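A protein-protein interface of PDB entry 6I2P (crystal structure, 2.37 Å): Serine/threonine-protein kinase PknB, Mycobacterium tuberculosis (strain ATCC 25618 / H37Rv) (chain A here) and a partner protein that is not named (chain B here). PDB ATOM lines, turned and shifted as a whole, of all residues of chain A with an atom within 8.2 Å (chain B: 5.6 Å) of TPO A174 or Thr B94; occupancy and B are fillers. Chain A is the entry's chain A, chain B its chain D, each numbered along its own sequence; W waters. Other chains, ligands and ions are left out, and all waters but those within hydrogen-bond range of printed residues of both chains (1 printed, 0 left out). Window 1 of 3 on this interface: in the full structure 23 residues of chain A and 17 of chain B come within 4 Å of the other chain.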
ATOM      1  N   MET A  23      32.386   1.115 -14.839  1.00  0.00           N
ATOM      2  CA  MET A  23      33.761   0.688 -14.565  1.00  0.00           C
ATOM      3  C   MET A  23      34.731   1.857 -14.785  1.00  0.00           C
ATOM      4  O   MET A  23      35.947   1.703 -14.656  1.00  0.00           O
ATOM      5  CB  MET A  23      34.126  -0.497 -15.484  1.00  0.00           C
ATOM      6  CG  MET A  23      34.247  -0.121 -16.960  1.00  0.00           C
ATOM      7  SD  MET A  23      34.831  -1.467 -18.006  1.00  0.00           S
ATOM      8  CE  MET A  23      33.309  -2.310 -18.297  1.00  0.00           C
ATOM      9  N   LYS A  41      37.750  10.118 -20.002  1.00  0.00           N
ATOM     10  CA  LYS A  41      37.098   8.936 -19.445  1.00  0.00           C
ATOM     11  C   LYS A  41      38.144   7.848 -19.373  1.00  0.00           C
ATOM     12  O   LYS A  41      38.783   7.501 -20.369  1.00  0.00           O
ATOM     13  CB  LYS A  41      35.885   8.485 -20.273  1.00  0.00           C
ATOM     14  CG  LYS A  41      35.088   7.357 -19.593  1.00  0.00           C
ATOM     15  CD  LYS A  41      34.069   6.701 -20.523  1.00  0.00           C
ATOM     16  CE  LYS A  41      32.746   7.415 -20.498  1.00  0.00           C
ATOM     17  NZ  LYS A  41      31.825   6.880 -21.519  1.00  0.00           N
ATOM     18  N   ARG A  56      37.503  -5.149 -21.522  1.00  0.00           N
ATOM     19  CA  ARG A  56      36.194  -4.531 -21.745  1.00  0.00           C
ATOM     20  C   ARG A  56      36.336  -3.034 -22.052  1.00  0.00           C
ATOM     21  O   ARG A  56      35.677  -2.550 -22.969  1.00  0.00           O
ATOM     22  CB  ARG A  56      35.261  -4.752 -20.545  1.00  0.00           C
ATOM     23  CG  ARG A  56      34.664  -6.162 -20.461  1.00  0.00           C
ATOM     24  CD  ARG A  56      34.125  -6.466 -19.061  1.00  0.00           C
ATOM     25  NE  ARG A  56      32.902  -5.709 -18.809  1.00  0.00           N
ATOM     26  CZ  ARG A  56      32.216  -5.628 -17.673  1.00  0.00           C
ATOM     27  NH1 ARG A  56      31.112  -4.892 -17.611  1.00  0.00           N
ATOM     28  NH2 ARG A  56      32.647  -6.252 -16.580  1.00  0.00           N
ATOM     29  N   ARG A  59      38.020  -2.185 -25.694  1.00  0.00           N
ATOM     30  CA  ARG A  59      37.004  -2.229 -26.757  1.00  0.00           C
ATOM     31  C   ARG A  59      36.238  -0.911 -26.831  1.00  0.00           C
ATOM     32  O   ARG A  59      35.982  -0.419 -27.927  1.00  0.00           O
ATOM     33  CB  ARG A  59      35.977  -3.337 -26.474  1.00  0.00           C
ATOM     34  CG  ARG A  59      36.393  -4.733 -26.847  1.00  0.00           C
ATOM     35  CD  ARG A  59      35.204  -5.634 -26.600  1.00  0.00           C
ATOM     36  NE  ARG A  59      35.454  -7.028 -26.964  1.00  0.00           N
ATOM     37  CZ  ARG A  59      36.044  -7.913 -26.169  1.00  0.00           C
ATOM     38  NH1 ARG A  59      36.483  -7.549 -24.967  1.00  0.00           N
ATOM     39  NH2 ARG A  59      36.212  -9.163 -26.571  1.00  0.00           N
ATOM     40  N   GLU A  60      35.826  -0.384 -25.656  1.00  0.00           N
ATOM     41  CA  GLU A  60      35.068   0.853 -25.488  1.00  0.00           C
ATOM     42  C   GLU A  60      35.846   2.044 -26.058  1.00  0.00           C
ATOM     43  O   GLU A  60      35.257   2.843 -26.788  1.00  0.00           O
ATOM     44  CB  GLU A  60      34.735   1.065 -24.000  1.00  0.00           C
ATOM     45  CG  GLU A  60      33.513   1.933 -23.743  1.00  0.00           C
ATOM     46  CD  GLU A  60      32.884   1.776 -22.369  1.00  0.00           C
ATOM     47  OE1 GLU A  60      32.603   0.626 -21.960  1.00  0.00           O
ATOM     48  OE2 GLU A  60      32.659   2.814 -21.707  1.00  0.00           O
ATOM     49  N   ASN A  63      35.962   1.708 -29.839  1.00  0.00           N
ATOM     50  CA  ASN A  63      34.637   1.905 -30.446  1.00  0.00           C
ATOM     51  C   ASN A  63      34.037   3.300 -30.243  1.00  0.00           C
ATOM     52  O   ASN A  63      32.955   3.569 -30.777  1.00  0.00           O
ATOM     53  CB  ASN A  63      33.638   0.828 -29.978  1.00  0.00           C
ATOM     54  CG  ASN A  63      33.814  -0.536 -30.605  1.00  0.00           C
ATOM     55  OD1 ASN A  63      34.193  -0.681 -31.770  1.00  0.00           O
ATOM     56  ND2 ASN A  63      33.517  -1.575 -29.844  1.00  0.00           N
ATOM     57  N   HIS A 137      22.182   5.242 -32.342  1.00  0.00           N
ATOM     58  CA  HIS A 137      22.684   5.424 -30.978  1.00  0.00           C
ATOM     59  C   HIS A 137      22.500   4.132 -30.160  1.00  0.00           C
ATOM     60  O   HIS A 137      23.473   3.624 -29.592  1.00  0.00           O
ATOM     61  CB  HIS A 137      21.985   6.609 -30.295  1.00  0.00           C
ATOM     62  CG  HIS A 137      22.618   6.998 -28.994  1.00  0.00           C
ATOM     63  ND1 HIS A 137      22.526   6.192 -27.879  1.00  0.00           N
ATOM     64  CD2 HIS A 137      23.344   8.094 -28.681  1.00  0.00           C
ATOM     65  CE1 HIS A 137      23.205   6.812 -26.932  1.00  0.00           C
ATOM     66  NE2 HIS A 137      23.699   7.965 -27.362  1.00  0.00           N
ATOM     67  N   ARG A 138      21.247   3.608 -30.116  1.00  0.00           N
ATOM     68  CA  ARG A 138      20.807   2.371 -29.436  1.00  0.00           C
ATOM     69  C   ARG A 138      20.642   2.479 -27.918  1.00  0.00           C
ATOM     70  O   ARG A 138      20.026   1.594 -27.316  1.00  0.00           O
ATOM     71  CB  ARG A 138      21.715   1.160 -29.760  1.00  0.00           C
ATOM     72  CG  ARG A 138      21.860   0.835 -31.229  1.00  0.00           C
ATOM     73  CD  ARG A 138      23.023  -0.112 -31.469  1.00  0.00           C
ATOM     74  NE  ARG A 138      23.384  -0.152 -32.886  1.00  0.00           N
ATOM     75  CZ  ARG A 138      22.830  -0.958 -33.785  1.00  0.00           C
ATOM     76  NH1 ARG A 138      23.206  -0.902 -35.054  1.00  0.00           N
ATOM     77  NH2 ARG A 138      21.887  -1.820 -33.423  1.00  0.00           N
ATOM     78  N   ASP A 139      21.192   3.532 -27.296  1.00  0.00           N
ATOM     79  CA  ASP A 139      21.148   3.693 -25.841  1.00  0.00           C
ATOM     80  C   ASP A 139      20.743   5.116 -25.408  1.00  0.00           C
ATOM     81  O   ASP A 139      21.341   5.701 -24.498  1.00  0.00           O
ATOM     82  CB  ASP A 139      22.494   3.238 -25.224  1.00  0.00           C
ATOM     83  CG  ASP A 139      22.481   2.967 -23.726  1.00  0.00           C
ATOM     84  OD1 ASP A 139      21.538   2.289 -23.249  1.00  0.00           O
ATOM     85  OD2 ASP A 139      23.427   3.414 -23.032  1.00  0.00           O
ATOM     86  N   LYS A 141      18.951   7.659 -23.430  1.00  0.00           N
ATOM     87  CA  LYS A 141      18.427   7.709 -22.069  1.00  0.00           C
ATOM     88  C   LYS A 141      18.808   9.055 -21.427  1.00  0.00           C
ATOM     89  O   LYS A 141      19.749   9.690 -21.913  1.00  0.00           O
ATOM     90  CB  LYS A 141      18.934   6.499 -21.239  1.00  0.00           C
ATOM     91  CG  LYS A 141      20.445   6.396 -21.054  1.00  0.00           C
ATOM     92  CD  LYS A 141      20.805   5.059 -20.444  1.00  0.00           C
ATOM     93  CE  LYS A 141      22.290   4.924 -20.204  1.00  0.00           C
ATOM     94  NZ  LYS A 141      22.656   3.573 -19.692  1.00  0.00           N
ATOM     95  N   ASP A 157      27.758   9.019 -25.812  1.00  0.00           N
ATOM     96  CA  ASP A 157      27.769   7.559 -25.940  1.00  0.00           C
ATOM     97  C   ASP A 157      27.246   7.061 -27.295  1.00  0.00           C
ATOM     98  O   ASP A 157      26.345   6.224 -27.358  1.00  0.00           O
ATOM     99  CB  ASP A 157      27.055   6.865 -24.752  1.00  0.00           C
ATOM    100  CG  ASP A 157      27.405   5.396 -24.582  1.00  0.00           C
ATOM    101  OD1 ASP A 157      28.603   5.090 -24.374  1.00  0.00           O
ATOM    102  OD2 ASP A 157      26.479   4.554 -24.649  1.00  0.00           O
ATOM    103  N   GLY A 159      28.270   4.914 -30.633  1.00  0.00           N
ATOM    104  CA  GLY A 159      29.250   3.895 -30.998  1.00  0.00           C
ATOM    105  C   GLY A 159      29.617   3.920 -32.467  1.00  0.00           C
ATOM    106  O   GLY A 159      28.857   4.457 -33.272  1.00  0.00           O
ATOM    107  N   VAL A 171      35.418  -4.241 -33.973  1.00  0.00           N
ATOM    108  CA  VAL A 171      35.435  -4.547 -32.541  1.00  0.00           C
ATOM    109  C   VAL A 171      33.995  -4.805 -32.034  1.00  0.00           C
ATOM    110  O   VAL A 171      33.057  -4.119 -32.460  1.00  0.00           O
ATOM    111  CB  VAL A 171      36.199  -3.439 -31.748  1.00  0.00           C
ATOM    112  CG1 VAL A 171      36.211  -3.719 -30.252  1.00  0.00           C
ATOM    113  CG2 VAL A 171      37.631  -3.278 -32.261  1.00  0.00           C
ATOM    114  N   TPO A 172      33.831  -5.817 -31.151  1.00  0.00           N
ATOM    115  CA  TPO A 172      32.543  -6.230 -30.587  1.00  0.00           C
ATOM    116  CB  TPO A 172      32.584  -7.627 -29.912  1.00  0.00           C
ATOM    117  CG2 TPO A 172      31.184  -8.267 -29.688  1.00  0.00           C
ATOM    118  OG1 TPO A 172      33.312  -8.550 -30.752  1.00  0.00           O
ATOM    119  P   TPO A 172      34.641  -9.032 -30.185  1.00  0.00           P
ATOM    120  O1P TPO A 172      35.626  -7.868 -29.945  1.00  0.00           O
ATOM    121  O2P TPO A 172      35.286  -9.958 -31.209  1.00  0.00           O
ATOM    122  O3P TPO A 172      34.424  -9.791 -28.877  1.00  0.00           O
ATOM    123  C   TPO A 172      31.944  -5.183 -29.655  1.00  0.00           C
ATOM    124  O   TPO A 172      32.651  -4.585 -28.852  1.00  0.00           O
ATOM    125  N   GLN A 173      30.629  -4.980 -29.771  1.00  0.00           N
ATOM    126  CA  GLN A 173      29.866  -4.044 -28.951  1.00  0.00           C
ATOM    127  C   GLN A 173      29.095  -4.789 -27.862  1.00  0.00           C
ATOM    128  O   GLN A 173      28.727  -5.951 -28.043  1.00  0.00           O
ATOM    129  CB  GLN A 173      28.915  -3.206 -29.821  1.00  0.00           C
ATOM    130  N   TPO A 174      28.857  -4.119 -26.729  1.00  0.00           N
ATOM    131  CA  TPO A 174      28.119  -4.693 -25.604  1.00  0.00           C
ATOM    132  CB  TPO A 174      28.476  -4.033 -24.253  1.00  0.00           C
ATOM    133  CG2 TPO A 174      29.636  -4.798 -23.632  1.00  0.00           C
ATOM    134  OG1 TPO A 174      28.903  -2.673 -24.381  1.00  0.00           O
ATOM    135  P   TPO A 174      27.889  -1.599 -23.882  1.00  0.00           P
ATOM    136  O1P TPO A 174      28.775  -0.443 -23.380  1.00  0.00           O
ATOM    137  O2P TPO A 174      27.065  -1.101 -25.083  1.00  0.00           O
ATOM    138  O3P TPO A 174      26.947  -2.041 -22.743  1.00  0.00           O
ATOM    139  C   TPO A 174      26.617  -4.711 -25.886  1.00  0.00           C
ATOM    140  O   TPO A 174      26.147  -3.965 -26.749  1.00  0.00           O
ATOM    141  N   ALA A 175      25.870  -5.574 -25.173  1.00  0.00           N
ATOM    142  CA  ALA A 175      24.418  -5.679 -25.327  1.00  0.00           C
ATOM    143  C   ALA A 175      23.743  -4.488 -24.628  1.00  0.00           C
ATOM    144  O   ALA A 175      23.982  -4.255 -23.440  1.00  0.00           O
ATOM    145  CB  ALA A 175      23.920  -7.000 -24.755  1.00  0.00           C
ATOM    146  N   ALA A 176      22.942  -3.709 -25.383  1.00  0.00           N
ATOM    147  CA  ALA A 176      22.226  -2.528 -24.872  1.00  0.00           C
ATOM    148  C   ALA A 176      21.046  -2.913 -23.966  1.00  0.00           C
ATOM    149  O   ALA A 176      20.575  -2.091 -23.174  1.00  0.00           O
ATOM    150  CB  ALA A 176      21.741  -1.666 -26.031  1.00  0.00           C
ATOM    151  N   VAL A 177      20.593  -4.176 -24.086  1.00  0.00           N
ATOM    152  CA  VAL A 177      19.481  -4.814 -23.368  1.00  0.00           C
ATOM    153  C   VAL A 177      19.669  -4.792 -21.831  1.00  0.00           C
ATOM    154  O   VAL A 177      18.680  -4.680 -21.101  1.00  0.00           O
ATOM    155  CB  VAL A 177      19.242  -6.248 -23.928  1.00  0.00           C
ATOM    156  CG1 VAL A 177      17.978  -6.878 -23.355  1.00  0.00           C
ATOM    157  CG2 VAL A 177      19.169  -6.234 -25.452  1.00  0.00           C
ATOM    158  N   ILE A 178      20.928  -4.875 -21.350  1.00  0.00           N
ATOM    159  CA  ILE A 178      21.242  -4.849 -19.916  1.00  0.00           C
ATOM    160  C   ILE A 178      20.964  -3.444 -19.323  1.00  0.00           C
ATOM    161  O   ILE A 178      21.201  -2.433 -19.993  1.00  0.00           O
ATOM    162  CB  ILE A 178      22.675  -5.408 -19.620  1.00  0.00           C
ATOM    163  CG1 ILE A 178      22.841  -5.832 -18.144  1.00  0.00           C
ATOM    164  CG2 ILE A 178      23.807  -4.474 -20.069  1.00  0.00           C
ATOM    165  CD1 ILE A 178      22.463  -7.295 -17.856  1.00  0.00           C
ATOM    166  N   GLY A 179      20.405  -3.415 -18.112  1.00  0.00           N
ATOM    167  CA  GLY A 179      20.050  -2.189 -17.403  1.00  0.00           C
ATOM    168  C   GLY A 179      18.640  -2.173 -16.841  1.00  0.00           C
ATOM    169  O   GLY A 179      18.070  -3.229 -16.546  1.00  0.00           O
ATOM    170  N   ARG B  82      31.263 -13.636 -35.873  1.00  0.00           N
ATOM    171  CA  ARG B  82      31.266 -12.520 -36.821  1.00  0.00           C
ATOM    172  C   ARG B  82      32.528 -12.512 -37.706  1.00  0.00           C
ATOM    173  O   ARG B  82      32.617 -11.692 -38.620  1.00  0.00           O
ATOM    174  CB  ARG B  82      31.085 -11.181 -36.070  1.00  0.00           C
ATOM    175  CG  ARG B  82      30.604 -10.012 -36.943  1.00  0.00           C
ATOM    176  CD  ARG B  82      30.212  -8.760 -36.175  1.00  0.00           C
ATOM    177  NE  ARG B  82      30.921  -8.613 -34.897  1.00  0.00           N
ATOM    178  CZ  ARG B  82      32.108  -8.035 -34.754  1.00  0.00           C
ATOM    179  NH1 ARG B  82      32.741  -7.531 -35.807  1.00  0.00           N
ATOM    180  NH2 ARG B  82      32.676  -7.963 -33.557  1.00  0.00           N
ATOM    181  N   ASP B  92      26.408  -9.365 -36.613  1.00  0.00           N
ATOM    182  CA  ASP B  92      25.713  -8.576 -35.598  1.00  0.00           C
ATOM    183  C   ASP B  92      26.798  -7.991 -34.687  1.00  0.00           C
ATOM    184  O   ASP B  92      27.686  -8.733 -34.275  1.00  0.00           O
ATOM    185  CB  ASP B  92      24.750  -9.512 -34.841  1.00  0.00           C
ATOM    186  CG  ASP B  92      24.179  -9.104 -33.496  1.00  0.00           C
ATOM    187  OD1 ASP B  92      24.628  -8.077 -32.934  1.00  0.00           O
ATOM    188  OD2 ASP B  92      23.308  -9.824 -32.996  1.00  0.00           O
ATOM    189  N   VAL B  93      26.711  -6.670 -34.369  1.00  0.00           N
ATOM    190  CA  VAL B  93      27.671  -5.902 -33.543  1.00  0.00           C
ATOM    191  C   VAL B  93      27.963  -6.543 -32.167  1.00  0.00           C
ATOM    192  O   VAL B  93      29.075  -6.389 -31.655  1.00  0.00           O
ATOM    193  CB  VAL B  93      27.313  -4.390 -33.380  1.00  0.00           C
ATOM    194  CG1 VAL B  93      27.410  -3.650 -34.707  1.00  0.00           C
ATOM    195  CG2 VAL B  93      25.941  -4.173 -32.731  1.00  0.00           C
ATOM    196  N   THR B  94      26.979  -7.249 -31.588  1.00  0.00           N
ATOM    197  CA  THR B  94      27.086  -7.897 -30.279  1.00  0.00           C
ATOM    198  C   THR B  94      27.704  -9.315 -30.356  1.00  0.00           C
ATOM    199  O   THR B  94      28.068  -9.865 -29.320  1.00  0.00           O
ATOM    200  CB  THR B  94      25.726  -7.875 -29.554  1.00  0.00           C
ATOM    201  OG1 THR B  94      24.772  -8.630 -30.296  1.00  0.00           O
ATOM    202  CG2 THR B  94      25.205  -6.452 -29.317  1.00  0.00           C
ATOM    203  N   VAL B  95      27.841  -9.892 -31.564  1.00  0.00           N
ATOM    204  CA  VAL B  95      28.448 -11.214 -31.759  1.00  0.00           C
ATOM    205  C   VAL B  95      29.966 -11.020 -31.870  1.00  0.00           C
ATOM    206  O   VAL B  95      30.423 -10.163 -32.627  1.00  0.00           O
ATOM    207  CB  VAL B  95      27.870 -11.995 -32.997  1.00  0.00           C
ATOM    208  CG1 VAL B  95      28.583 -13.333 -33.206  1.00  0.00           C
ATOM    209  CG2 VAL B  95      26.363 -12.215 -32.878  1.00  0.00           C
ATOM    210  N   SER B  96      30.743 -11.819 -31.122  1.00  0.00           N
ATOM    211  CA  SER B  96      32.200 -11.788 -31.176  1.00  0.00           C
ATOM    212  C   SER B  96      32.659 -12.479 -32.451  1.00  0.00           C
ATOM    213  O   SER B  96      31.963 -13.371 -32.936  1.00  0.00           O
ATOM    214  CB  SER B  96      32.795 -12.507 -29.967  1.00  0.00           C
ATOM    215  OG  SER B  96      32.515 -11.810 -28.767  1.00  0.00           O
ATOM    216  N   HIS B  99      32.973 -16.445 -31.342  1.00  0.00           N
ATOM    217  CA  HIS B  99      31.943 -16.430 -30.298  1.00  0.00           C
ATOM    218  C   HIS B  99      31.740 -17.800 -29.688  1.00  0.00           C
ATOM    219  O   HIS B  99      31.939 -17.973 -28.483  1.00  0.00           O
ATOM    220  CB  HIS B  99      30.604 -15.865 -30.838  1.00  0.00           C
ATOM    221  CG  HIS B  99      29.611 -15.504 -29.768  1.00  0.00           C
ATOM    222  ND1 HIS B  99      29.231 -14.189 -29.557  1.00  0.00           N
ATOM    223  CD2 HIS B  99      28.959 -16.292 -28.879  1.00  0.00           C
ATOM    224  CE1 HIS B  99      28.352 -14.220 -28.568  1.00  0.00           C
ATOM    225  NE2 HIS B  99      28.162 -15.463 -28.123  1.00  0.00           N
ATOM    226  N   LEU B 117      32.271 -11.766 -25.677  1.00  0.00           N
ATOM    227  CA  LEU B 117      32.032 -10.593 -24.848  1.00  0.00           C
ATOM    228  C   LEU B 117      30.671 -10.662 -24.136  1.00  0.00           C
ATOM    229  O   LEU B 117      30.593 -10.407 -22.938  1.00  0.00           O
ATOM    230  CB  LEU B 117      32.132  -9.313 -25.725  1.00  0.00           C
ATOM    231  CG  LEU B 117      31.796  -7.962 -25.071  1.00  0.00           C
ATOM    232  CD1 LEU B 117      32.800  -7.595 -23.992  1.00  0.00           C
ATOM    233  CD2 LEU B 117      31.684  -6.869 -26.114  1.00  0.00           C
ATOM    234  N   ASN B 118      29.608 -10.997 -24.877  1.00  0.00           N
ATOM    235  CA  ASN B 118      28.241 -11.010 -24.350  1.00  0.00           C
ATOM    236  C   ASN B 118      27.701 -12.410 -23.970  1.00  0.00           C
ATOM    237  O   ASN B 118      26.586 -12.510 -23.442  1.00  0.00           O
ATOM    238  CB  ASN B 118      27.309 -10.285 -25.321  1.00  0.00           C
ATOM    239  CG  ASN B 118      27.736  -8.851 -25.598  1.00  0.00           C
ATOM    240  OD1 ASN B 118      27.902  -8.022 -24.692  1.00  0.00           O
ATOM    241  ND2 ASN B 118      27.936  -8.527 -26.865  1.00  0.00           N
ATOM    242  N   GLY B 141      24.584 -13.297 -29.521  1.00  0.00           N
ATOM    243  CA  GLY B 141      24.350 -11.883 -29.784  1.00  0.00           C
ATOM    244  C   GLY B 141      22.871 -11.584 -29.689  1.00  0.00           C
ATOM    245  O   GLY B 141      22.243 -11.858 -28.663  1.00  0.00           O
ATOM    246  N   LYS B 142      22.301 -11.078 -30.785  1.00  0.00           N
ATOM    247  CA  LYS B 142      20.873 -10.800 -30.912  1.00  0.00           C
ATOM    248  C   LYS B 142      20.208 -11.923 -31.729  1.00  0.00           C
ATOM    249  O   LYS B 142      19.020 -11.828 -32.034  1.00  0.00           O
ATOM    250  CB  LYS B 142      20.622  -9.422 -31.562  1.00  0.00           C
ATOM    251  CG  LYS B 142      21.008  -8.224 -30.708  1.00  0.00           C
ATOM    252  CD  LYS B 142      20.657  -6.928 -31.427  1.00  0.00           C
ATOM    253  CE  LYS B 142      21.867  -6.084 -31.757  1.00  0.00           C
ATOM    254  NZ  LYS B 142      21.511  -4.927 -32.614  1.00  0.00           N
HETATM  255  O   HOH W   1      20.295  -2.459 -30.549  1.00  0.00           O
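The guanidinium group (NH2) of Arg B82 sits at hydrogen-bond distance from OG1 of TPO A172 (2.9 Å). O3P of TPO A172 sits at hydrogen-bond distance from the side-chain hydroxyl of Ser B96 (2.8 Å). N of Gln A173 lies within hydrogen-bond range of O of Val B93 (2.8 Å). O of Gln A173 lies within hydrogen-bond range of ND2 of Asn B118 (2.9 Å). The side-chain amide oxygen (OD1) of Asn B118 lies within hydrogen-bond range of the backbone NH (N) of Ala A175 (3.2 Å). NH2 of Arg A138 lies close to NZ of Lys B142 (3.2 Å).
The guanidinium group (NH2) of Arg A59 sits close to O3P of TPO A172, 3.0 Å away. O of TPO A172 is in hydrogen-bond range of the side-chain amide nitrogen (ND2) of Asn A63, 3.3 Å away. The backbone NH (N) of Arg B82 is in hydrogen-bond range of the backbone carbonyl oxygen (O) of Ser B96 (3.0 Å). The side-chain hydroxyl (OG1) of Thr B94 is in hydrogen-bond range of the side-chain carboxylate (OD1) of Asp B92, 2.7 Å away. The side-chain amide nitrogen of Asn B118 is in hydrogen-bond range of the backbone carbonyl oxygen of Thr B94 (2.8 Å). OG of Ser B96 is in hydrogen-bond range of N of Leu B117 (3.1 Å).
CD of Arg A59 touches CD2 of Leu B117, at 3.8 Å. Arg B82 touches Val A171. Val B93 touches TPO A172 (O to CG2, 3.4 Å). TPO A172 touches Thr B94. Leu B117 touches TPO A172. Thr B94 touches Gln A173. O of Gln A173 touches CD2 of Leu B117, 3.6 Å away. TPO A174 touches Thr B94 (O to CG2, 3.7 Å). TPO A174 touches Leu B117 (CG2 to CD2, 3.8 Å). OD1 of Asn B118 touches CA of TPO A174 (3.5 Å).
TPO A174 touches just these residues of chain B: Thr B94 (3.7 Å), Leu B117 (3.8 Å) and Asn B118 (3.5 Å). Of the printed residues of chain B, Ala A175 touches Asn B118. Of chain A, only TPO A172 (3.5 Å), Gln A173 (3.4 Å) and TPO A174 (3.7 Å) come within 4 Å of Thr B94. Of the printed residues of chain A, Lys B142 touches Arg A138 (3.2 Å). The nearest printed residue of chain B that does not touch TPO A172 is Asn B118 (4.3 Å).
Of the 11 printed residues of chain B, 8 touch a printed residue of chain A. Hydrophobic or aromatic side chains of chain B within 4 Å of the printed part of chain A: Leu B117. Of the 21 printed residues of chain A, 7 touch a printed residue of chain B. Among the printed residues, 17 pairs touch across the chains. Among the printed residues, no Asp or Glu carboxylate lies within 4 Å of a Lys or Arg side-chain nitrogen of the other chain.
Water W1 bridges the guanidinium group (NH2) of Arg A138 (3.3 Å) and the side-chain amino group (NZ) of Lys B142 (3.4 Å).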
